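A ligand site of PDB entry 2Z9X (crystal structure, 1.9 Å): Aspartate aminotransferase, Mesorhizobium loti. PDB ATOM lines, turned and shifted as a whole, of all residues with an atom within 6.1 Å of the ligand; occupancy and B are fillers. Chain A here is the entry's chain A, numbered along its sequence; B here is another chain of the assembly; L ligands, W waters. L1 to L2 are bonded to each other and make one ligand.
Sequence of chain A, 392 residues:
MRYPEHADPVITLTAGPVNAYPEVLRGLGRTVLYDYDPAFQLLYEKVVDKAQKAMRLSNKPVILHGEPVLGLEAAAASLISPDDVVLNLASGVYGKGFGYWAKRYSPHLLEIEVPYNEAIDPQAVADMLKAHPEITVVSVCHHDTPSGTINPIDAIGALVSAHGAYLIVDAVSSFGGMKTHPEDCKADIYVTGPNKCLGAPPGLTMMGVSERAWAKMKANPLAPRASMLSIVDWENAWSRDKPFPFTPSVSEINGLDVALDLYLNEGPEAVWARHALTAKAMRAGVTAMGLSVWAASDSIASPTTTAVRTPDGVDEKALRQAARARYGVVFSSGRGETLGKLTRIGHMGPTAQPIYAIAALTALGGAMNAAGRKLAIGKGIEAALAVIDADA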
ATOM      1  N   ALA A  15      34.964  -9.842  19.275  1.00  0.00           N
ATOM      2  CA  ALA A  15      33.832  -9.287  20.014  1.00  0.00           C
ATOM      3  C   ALA A  15      32.517  -9.347  19.230  1.00  0.00           C
ATOM      4  O   ALA A  15      31.578  -8.642  19.539  1.00  0.00           O
ATOM      5  CB  ALA A  15      34.157  -7.821  20.440  1.00  0.00           C
ATOM      6  N   GLY A  16      32.469 -10.187  18.189  1.00  0.00           N
ATOM      7  CA  GLY A  16      31.222 -10.412  17.445  1.00  0.00           C
ATOM      8  C   GLY A  16      31.482 -10.326  15.946  1.00  0.00           C
ATOM      9  O   GLY A  16      31.864  -9.282  15.437  1.00  0.00           O
ATOM     10  N   PRO A  17      31.306 -11.451  15.222  1.00  0.00           N
ATOM     11  CA  PRO A  17      30.932 -12.768  15.722  1.00  0.00           C
ATOM     12  C   PRO A  17      32.004 -13.344  16.648  1.00  0.00           C
ATOM     13  O   PRO A  17      33.115 -12.798  16.721  1.00  0.00           O
ATOM     14  CB  PRO A  17      30.847 -13.642  14.449  1.00  0.00           C
ATOM     15  CG  PRO A  17      31.479 -12.898  13.373  1.00  0.00           C
ATOM     16  CD  PRO A  17      31.525 -11.442  13.757  1.00  0.00           C
ATOM     17  N   GLU A  67      19.854 -11.800  11.933  1.00  0.00           N
ATOM     18  CA  GLU A  67      20.714 -11.385  13.047  1.00  0.00           C
ATOM     19  C   GLU A  67      20.194 -10.054  13.638  1.00  0.00           C
ATOM     20  O   GLU A  67      19.342  -9.373  13.022  1.00  0.00           O
ATOM     21  CB  GLU A  67      22.202 -11.385  12.645  1.00  0.00           C
ATOM     22  CG  GLU A  67      22.740 -10.136  11.966  1.00  0.00           C
ATOM     23  CD  GLU A  67      23.470  -9.215  12.951  1.00  0.00           C
ATOM     24  OE1 GLU A  67      23.198  -8.018  12.921  1.00  0.00           O
ATOM     25  OE2 GLU A  67      24.347  -9.651  13.715  1.00  0.00           O
ATOM     26  N   PRO A  68      20.643  -9.700  14.848  1.00  0.00           N
ATOM     27  CA  PRO A  68      20.004  -8.605  15.595  1.00  0.00           C
ATOM     28  C   PRO A  68      19.825  -7.215  14.952  1.00  0.00           C
ATOM     29  O   PRO A  68      18.969  -6.481  15.439  1.00  0.00           O
ATOM     30  CB  PRO A  68      20.861  -8.487  16.862  1.00  0.00           C
ATOM     31  CG  PRO A  68      21.272  -9.899  17.120  1.00  0.00           C
ATOM     32  CD  PRO A  68      21.676 -10.360  15.680  1.00  0.00           C
ATOM     33  N   VAL A  69      20.560  -6.855  13.905  1.00  0.00           N
ATOM     34  CA  VAL A  69      20.225  -5.575  13.209  1.00  0.00           C
ATOM     35  C   VAL A  69      18.787  -5.630  12.701  1.00  0.00           C
ATOM     36  O   VAL A  69      18.145  -4.589  12.564  1.00  0.00           O
ATOM     37  CB  VAL A  69      21.168  -5.181  12.048  1.00  0.00           C
ATOM     38  CG1 VAL A  69      22.557  -4.819  12.564  1.00  0.00           C
ATOM     39  CG2 VAL A  69      21.213  -6.280  10.953  1.00  0.00           C
ATOM     40  N   LEU A  72      16.629  -4.524  15.717  1.00  0.00           N
ATOM     41  CA  LEU A  72      16.764  -3.085  15.929  1.00  0.00           C
ATOM     42  C   LEU A  72      15.963  -2.273  14.923  1.00  0.00           C
ATOM     43  O   LEU A  72      15.216  -1.368  15.300  1.00  0.00           O
ATOM     44  CB  LEU A  72      18.240  -2.665  15.920  1.00  0.00           C
ATOM     45  CG  LEU A  72      19.115  -3.284  17.017  1.00  0.00           C
ATOM     46  CD1 LEU A  72      20.570  -2.952  16.732  1.00  0.00           C
ATOM     47  CD2 LEU A  72      18.672  -2.863  18.454  1.00  0.00           C
ATOM     48  N   TYR A  94      26.857   2.107  17.862  1.00  0.00           N
ATOM     49  CA  TYR A  94      25.479   1.567  17.772  1.00  0.00           C
ATOM     50  C   TYR A  94      24.405   2.520  18.293  1.00  0.00           C
ATOM     51  O   TYR A  94      23.352   2.639  17.700  1.00  0.00           O
ATOM     52  CB  TYR A  94      25.350   0.164  18.387  1.00  0.00           C
ATOM     53  CG  TYR A  94      25.934  -0.852  17.439  1.00  0.00           C
ATOM     54  CD1 TYR A  94      25.137  -1.444  16.445  1.00  0.00           C
ATOM     55  CD2 TYR A  94      27.280  -1.176  17.511  1.00  0.00           C
ATOM     56  CE1 TYR A  94      25.706  -2.369  15.537  1.00  0.00           C
ATOM     57  CE2 TYR A  94      27.846  -2.078  16.636  1.00  0.00           C
ATOM     58  CZ  TYR A  94      27.066  -2.658  15.647  1.00  0.00           C
ATOM     59  OH  TYR A  94      27.669  -3.558  14.781  1.00  0.00           O
ATOM     60  N   CYS A 141      21.649   1.878  23.994  1.00  0.00           N
ATOM     61  CA  CYS A 141      22.452   0.682  23.783  1.00  0.00           C
ATOM     62  C   CYS A 141      23.143   0.332  25.130  1.00  0.00           C
ATOM     63  O   CYS A 141      23.791   1.192  25.713  1.00  0.00           O
ATOM     64  CB  CYS A 141      23.495   0.956  22.696  1.00  0.00           C
ATOM     65  SG  CYS A 141      24.535  -0.462  22.267  1.00  0.00           S
ATOM     66  N   HIS A 143      25.625  -2.341  25.842  1.00  0.00           N
ATOM     67  CA  HIS A 143      27.044  -2.458  25.588  1.00  0.00           C
ATOM     68  C   HIS A 143      27.300  -1.986  24.162  1.00  0.00           C
ATOM     69  O   HIS A 143      26.958  -2.684  23.191  1.00  0.00           O
ATOM     70  CB  HIS A 143      27.480  -3.917  25.843  1.00  0.00           C
ATOM     71  CG  HIS A 143      28.908  -4.255  25.483  1.00  0.00           C
ATOM     72  ND1 HIS A 143      29.939  -3.324  25.450  1.00  0.00           N
ATOM     73  CD2 HIS A 143      29.468  -5.444  25.178  1.00  0.00           C
ATOM     74  CE1 HIS A 143      31.059  -3.943  25.116  1.00  0.00           C
ATOM     75  NE2 HIS A 143      30.801  -5.220  24.955  1.00  0.00           N
ATOM     76  N   ASP A 144      27.868  -0.788  24.020  1.00  0.00           N
ATOM     77  CA  ASP A 144      28.152  -0.281  22.675  1.00  0.00           C
ATOM     78  C   ASP A 144      29.482  -0.855  22.254  1.00  0.00           C
ATOM     79  O   ASP A 144      30.541  -0.262  22.485  1.00  0.00           O
ATOM     80  CB  ASP A 144      28.118   1.238  22.618  1.00  0.00           C
ATOM     81  CG  ASP A 144      27.792   1.772  21.216  1.00  0.00           C
ATOM     82  OD1 ASP A 144      28.376   1.236  20.247  1.00  0.00           O
ATOM     83  OD2 ASP A 144      26.948   2.694  21.086  1.00  0.00           O
ATOM     84  N   THR A 145      29.408  -2.027  21.629  1.00  0.00           N
ATOM     85  CA  THR A 145      30.518  -2.961  21.551  1.00  0.00           C
ATOM     86  C   THR A 145      31.831  -2.346  20.989  1.00  0.00           C
ATOM     87  O   THR A 145      32.909  -2.609  21.519  1.00  0.00           O
ATOM     88  CB  THR A 145      30.093  -4.276  20.823  1.00  0.00           C
ATOM     89  OG1 THR A 145      28.717  -4.576  21.122  1.00  0.00           O
ATOM     90  CG2 THR A 145      30.979  -5.439  21.284  1.00  0.00           C
ATOM     91  N   PRO A 146      31.752  -1.566  19.893  1.00  0.00           N
ATOM     92  CA  PRO A 146      32.978  -0.948  19.325  1.00  0.00           C
ATOM     93  C   PRO A 146      33.744  -0.036  20.289  1.00  0.00           C
ATOM     94  O   PRO A 146      34.865   0.359  19.990  1.00  0.00           O
ATOM     95  CB  PRO A 146      32.438  -0.160  18.116  1.00  0.00           C
ATOM     96  CG  PRO A 146      31.158  -0.907  17.725  1.00  0.00           C
ATOM     97  CD  PRO A 146      30.564  -1.312  19.050  1.00  0.00           C
ATOM     98  N   ASP A 170      19.091  -2.067  23.127  1.00  0.00           N
ATOM     99  CA  ASP A 170      19.993  -2.973  22.426  1.00  0.00           C
ATOM    100  C   ASP A 170      20.886  -3.639  23.497  1.00  0.00           C
ATOM    101  O   ASP A 170      21.795  -2.995  24.041  1.00  0.00           O
ATOM    102  CB  ASP A 170      20.868  -2.170  21.451  1.00  0.00           C
ATOM    103  CG  ASP A 170      21.953  -3.005  20.784  1.00  0.00           C
ATOM    104  OD1 ASP A 170      22.457  -2.580  19.716  1.00  0.00           O
ATOM    105  OD2 ASP A 170      22.324  -4.060  21.345  1.00  0.00           O
ATOM    106  N   VAL A 172      22.381  -6.689  22.732  1.00  0.00           N
ATOM    107  CA  VAL A 172      22.928  -7.757  21.882  1.00  0.00           C
ATOM    108  C   VAL A 172      24.235  -8.338  22.427  1.00  0.00           C
ATOM    109  O   VAL A 172      24.452  -9.560  22.385  1.00  0.00           O
ATOM    110  CB  VAL A 172      23.122  -7.243  20.443  1.00  0.00           C
ATOM    111  CG1 VAL A 172      23.988  -8.223  19.601  1.00  0.00           C
ATOM    112  CG2 VAL A 172      21.768  -6.992  19.796  1.00  0.00           C
ATOM    113  N   SER A 173      25.108  -7.457  22.932  1.00  0.00           N
ATOM    114  CA  SER A 173      26.444  -7.868  23.375  1.00  0.00           C
ATOM    115  C   SER A 173      26.630  -7.880  24.889  1.00  0.00           C
ATOM    116  O   SER A 173      27.768  -7.902  25.351  1.00  0.00           O
ATOM    117  CB  SER A 173      27.502  -6.991  22.724  1.00  0.00           C
ATOM    118  OG  SER A 173      27.289  -5.606  22.971  1.00  0.00           O
ATOM    119  N   LYS A 196      26.815 -13.646  20.757  1.00  0.00           N
ATOM    120  CA  LYS A 196      27.823 -13.042  21.602  1.00  0.00           C
ATOM    121  C   LYS A 196      27.998 -13.918  22.849  1.00  0.00           C
ATOM    122  O   LYS A 196      28.594 -14.992  22.765  1.00  0.00           O
ATOM    123  CB  LYS A 196      27.458 -11.580  21.925  1.00  0.00           C
ATOM    124  CG  LYS A 196      27.780 -10.624  20.753  1.00  0.00           C
ATOM    125  CD  LYS A 196      26.751 -10.774  19.608  1.00  0.00           C
ATOM    126  CE  LYS A 196      27.124  -9.912  18.394  1.00  0.00           C
ATOM    127  NZ  LYS A 196      26.145 -10.096  17.271  1.00  0.00           N
ATOM    128  N   SER A 332      39.362  -8.340  17.501  1.00  0.00           N
ATOM    129  CA  SER A 332      38.480  -7.470  16.736  1.00  0.00           C
ATOM    130  C   SER A 332      39.089  -6.078  16.536  1.00  0.00           C
ATOM    131  O   SER A 332      39.784  -5.531  17.414  1.00  0.00           O
ATOM    132  CB  SER A 332      37.130  -7.314  17.423  1.00  0.00           C
ATOM    133  OG  SER A 332      36.299  -8.439  17.207  1.00  0.00           O
ATOM    134  N   SER A 333      38.787  -5.504  15.376  1.00  0.00           N
ATOM    135  CA  SER A 333      39.044  -4.102  15.119  1.00  0.00           C
ATOM    136  C   SER A 333      37.971  -3.301  15.842  1.00  0.00           C
ATOM    137  O   SER A 333      37.015  -3.882  16.398  1.00  0.00           O
ATOM    138  CB  SER A 333      38.963  -3.831  13.612  1.00  0.00           C
ATOM    139  OG  SER A 333      37.634  -3.942  13.131  1.00  0.00           O
ATOM    140  N   GLY A 334      38.122  -1.971  15.859  1.00  0.00           N
ATOM    141  CA  GLY A 334      37.007  -1.089  16.184  1.00  0.00           C
ATOM    142  C   GLY A 334      35.993  -1.087  15.053  1.00  0.00           C
ATOM    143  O   GLY A 334      36.052  -1.923  14.143  1.00  0.00           O
ATOM    144  N   ARG A 335      35.072  -0.128  15.097  1.00  0.00           N
ATOM    145  CA  ARG A 335      34.023   0.015  14.074  1.00  0.00           C
ATOM    146  C   ARG A 335      33.699   1.502  13.973  1.00  0.00           C
ATOM    147  O   ARG A 335      33.694   2.207  14.976  1.00  0.00           O
ATOM    148  CB  ARG A 335      32.785  -0.793  14.482  1.00  0.00           C
ATOM    149  CG  ARG A 335      31.654  -0.746  13.481  1.00  0.00           C
ATOM    150  CD  ARG A 335      30.492  -1.637  13.830  1.00  0.00           C
ATOM    151  NE  ARG A 335      29.478  -1.532  12.776  1.00  0.00           N
ATOM    152  CZ  ARG A 335      29.359  -2.395  11.771  1.00  0.00           C
ATOM    153  NH1 ARG A 335      30.162  -3.453  11.699  1.00  0.00           N
ATOM    154  NH2 ARG A 335      28.432  -2.215  10.832  1.00  0.00           N
ATOM    155  N   ARG A 344      39.835  -4.628  20.093  1.00  0.00           N
ATOM    156  CA  ARG A 344      38.892  -5.294  21.017  1.00  0.00           C
ATOM    157  C   ARG A 344      39.235  -6.749  21.244  1.00  0.00           C
ATOM    158  O   ARG A 344      39.507  -7.518  20.304  1.00  0.00           O
ATOM    159  CB  ARG A 344      37.439  -5.162  20.533  1.00  0.00           C
ATOM    160  CG  ARG A 344      36.891  -3.740  20.593  1.00  0.00           C
ATOM    161  CD  ARG A 344      35.466  -3.678  20.070  1.00  0.00           C
ATOM    162  NE  ARG A 344      35.358  -3.882  18.615  1.00  0.00           N
ATOM    163  CZ  ARG A 344      34.219  -4.129  17.960  1.00  0.00           C
ATOM    164  NH1 ARG A 344      33.062  -4.293  18.622  1.00  0.00           N
ATOM    165  NH2 ARG A 344      34.235  -4.250  16.647  1.00  0.00           N
ATOM    166  N   TYR B  34      35.591 -15.155  13.182  1.00  0.00           N
ATOM    167  CA  TYR B  34      35.352 -13.713  13.041  1.00  0.00           C
ATOM    168  C   TYR B  34      35.159 -13.421  11.554  1.00  0.00           C
ATOM    169  O   TYR B  34      35.934 -13.932  10.725  1.00  0.00           O
ATOM    170  CB  TYR B  34      36.609 -12.996  13.499  1.00  0.00           C
ATOM    171  CG  TYR B  34      36.604 -11.466  13.522  1.00  0.00           C
ATOM    172  CD1 TYR B  34      37.770 -10.772  13.176  1.00  0.00           C
ATOM    173  CD2 TYR B  34      35.493 -10.734  13.983  1.00  0.00           C
ATOM    174  CE1 TYR B  34      37.835  -9.400  13.258  1.00  0.00           C
ATOM    175  CE2 TYR B  34      35.542  -9.312  14.025  1.00  0.00           C
ATOM    176  CZ  TYR B  34      36.729  -8.682  13.670  1.00  0.00           C
ATOM    177  OH  TYR B  34      36.844  -7.321  13.699  1.00  0.00           O
ATOM    178  N   ASP B  35      34.192 -12.583  11.207  1.00  0.00           N
ATOM    179  CA  ASP B  35      33.913 -12.343   9.769  1.00  0.00           C
ATOM    180  C   ASP B  35      34.980 -11.529   9.068  1.00  0.00           C
ATOM    181  O   ASP B  35      35.087 -11.565   7.823  1.00  0.00           O
ATOM    182  CB  ASP B  35      32.490 -11.786   9.511  1.00  0.00           C
ATOM    183  CG  ASP B  35      32.149 -10.558  10.359  1.00  0.00           C
ATOM    184  OD1 ASP B  35      32.893 -10.224  11.286  1.00  0.00           O
ATOM    185  OD2 ASP B  35      31.109  -9.923  10.066  1.00  0.00           O
ATOM    186  N   THR B 247      26.568  -8.410  10.120  1.00  0.00           N
ATOM    187  CA  THR B 247      27.250  -9.700  10.289  1.00  0.00           C
ATOM    188  C   THR B 247      26.592 -10.847   9.445  1.00  0.00           C
ATOM    189  O   THR B 247      25.391 -11.134   9.598  1.00  0.00           O
ATOM    190  CB  THR B 247      27.367 -10.062  11.788  1.00  0.00           C
ATOM    191  OG1 THR B 247      27.934  -8.947  12.500  1.00  0.00           O
ATOM    192  CG2 THR B 247      28.217 -11.315  11.996  1.00  0.00           C
HETATM  193  N1  LIG L   1      28.443  -5.594  16.399  1.00  0.00           N
HETATM  194  C1  LIG L   1      29.669  -6.221  15.845  1.00  0.00           C
HETATM  195  C2  LIG L   1      30.892  -5.377  16.266  1.00  0.00           C
HETATM  196  O1  LIG L   1      30.760  -4.708  17.334  1.00  0.00           O
HETATM  197  C3  LIG L   1      29.517  -6.313  14.294  1.00  0.00           C
HETATM  198  O2  LIG L   1      31.936  -5.445  15.586  1.00  0.00           O
HETATM  199  O1  LG2 L   2      24.613  -7.924  15.822  1.00  0.00           O
HETATM  200  C1  LG2 L   2      24.379  -6.534  15.560  1.00  0.00           C
HETATM  201  C2  LG2 L   2      24.872  -5.754  16.801  1.00  0.00           C
HETATM  202  C3  LG2 L   2      23.932  -4.980  17.482  1.00  0.00           C
HETATM  203  N1  LG2 L   2      24.249  -4.285  18.563  1.00  0.00           N
HETATM  204  C4  LG2 L   2      25.485  -4.261  19.043  1.00  0.00           C
HETATM  205  C5  LG2 L   2      26.466  -5.039  18.415  1.00  0.00           C
HETATM  206  C6  LG2 L   2      26.190  -5.782  17.263  1.00  0.00           C
HETATM  207  C7  LG2 L   2      27.331  -6.565  16.605  1.00  0.00           C
HETATM  208  O2  LG2 L   2      27.720  -5.066  18.860  1.00  0.00           O
HETATM  209  C8  LG2 L   2      25.779  -3.428  20.308  1.00  0.00           C
HETATM  210  O   HOH W   1      29.049  -7.573  19.010  1.00  0.00           O
HETATM  211  O   HOH W   2      25.835  -7.105  12.571  1.00  0.00           O
HETATM  212  O   HOH W   3      30.126  -8.018  11.299  1.00  0.00           O
HETATM  213  O   HOH W   4      33.835  -7.659  16.553  1.00  0.00           O
HETATM  214  O   HOH W   5      28.344  -9.570  15.282  1.00  0.00           O
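OG1 of Thr 145 sits at hydrogen-bond distance from O2 of LG2 L2 (2.5 Å). NH1 of Arg 344 lies within salt-bridge range of O1 of LIG L1, 2.7 Å away. The side-chain hydroxyl (OH) of Tyr 94 sits at hydrogen-bond distance from a nitrogen (N1) of LIG L1 (2.7 Å). The side-chain carboxylate (OD1) of Asp 170 sits at hydrogen-bond distance from a nitrogen (N1) of LG2 L2 (2.7 Å). An oxygen (O1) of LG2 L2 is in hydrogen-bond range of the side-chain carboxylate of Glu 67, at 2.7 Å. The side-chain amino group of Lys 196 lies within hydrogen-bond range of an oxygen (O1) of LG2 L2, 3.0 Å away.
Merely in contact with the ligand: Gly 16, Pro 68, Val 69, Leu 72, Cys 141, His 143, Pro 146, Val 172, Ser 173, Arg 335 and Thr 247 of chain B. Hydrophobic or aromatic side chains within 4 Å of the ligand: Pro 68, Val 69, Leu 72, Tyr 94, Pro 146 and Val 172. Within 4 Å of the ligand: Gly 16, Glu 67, Pro 68, Val 69, Leu 72, Tyr 94, Cys 141, His 143, Thr 145, Pro 146, Asp 170, Val 172, Ser 173, Lys 196, Arg 335, Arg 344 and Thr 247 of chain B. The nearest printed residue that does not touch the ligand is Ala 15 (4.6 Å).
Water W1 bridges the backbone carbonyl oxygen of Ala 15 and an oxygen (O2) of LG2 L2. Water W4 lies within hydrogen-bond range of OG of Ser 332, O of Gly 16, O2 of LIG L1 and NH2 of Arg 344. Water W2 lies within hydrogen-bond range of OG1 of Thr 247 of chain B (2.8 Å) and OE1 of Glu 67 (2.8 Å). Water W5 lies within hydrogen-bond range of OG1 of Thr 247 of chain B (2.9 Å) and NZ of Lys 196 (3.0 Å). Water W3 bridges the side-chain carboxylate of Asp 35 of chain B (2.5 Å) and the side-chain hydroxyl of Thr 247 of chain B (2.7 Å).
The side-chain hydroxyl of Ser 173 sits at hydrogen-bond distance from the side-chain hydroxyl of Thr 145, at 2.6 Å. The backbone carbonyl oxygen of Ser 333 sits at hydrogen-bond distance from the guanidinium group of Arg 344 (2.8 Å). N of Arg 344 is in hydrogen-bond range of O of Ser 332, 2.8 Å away. The side-chain carboxylate (OD2) of Asp 170 sits at hydrogen-bond distance from the backbone NH (N) of Val 172 (3.0 Å). The side-chain carboxylate (OE1) of Glu 67 lies within hydrogen-bond range of the backbone NH (N) of Val 69. OG of Ser 173 is in hydrogen-bond range of O of His 143 (2.9 Å). O of His 143 lies within hydrogen-bond range of SG of Cys 141 (3.4 Å). The backbone NH (N) of Asp 144 sits close to the side-chain sulfur (SG) of Cys 141 (3.8 Å).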
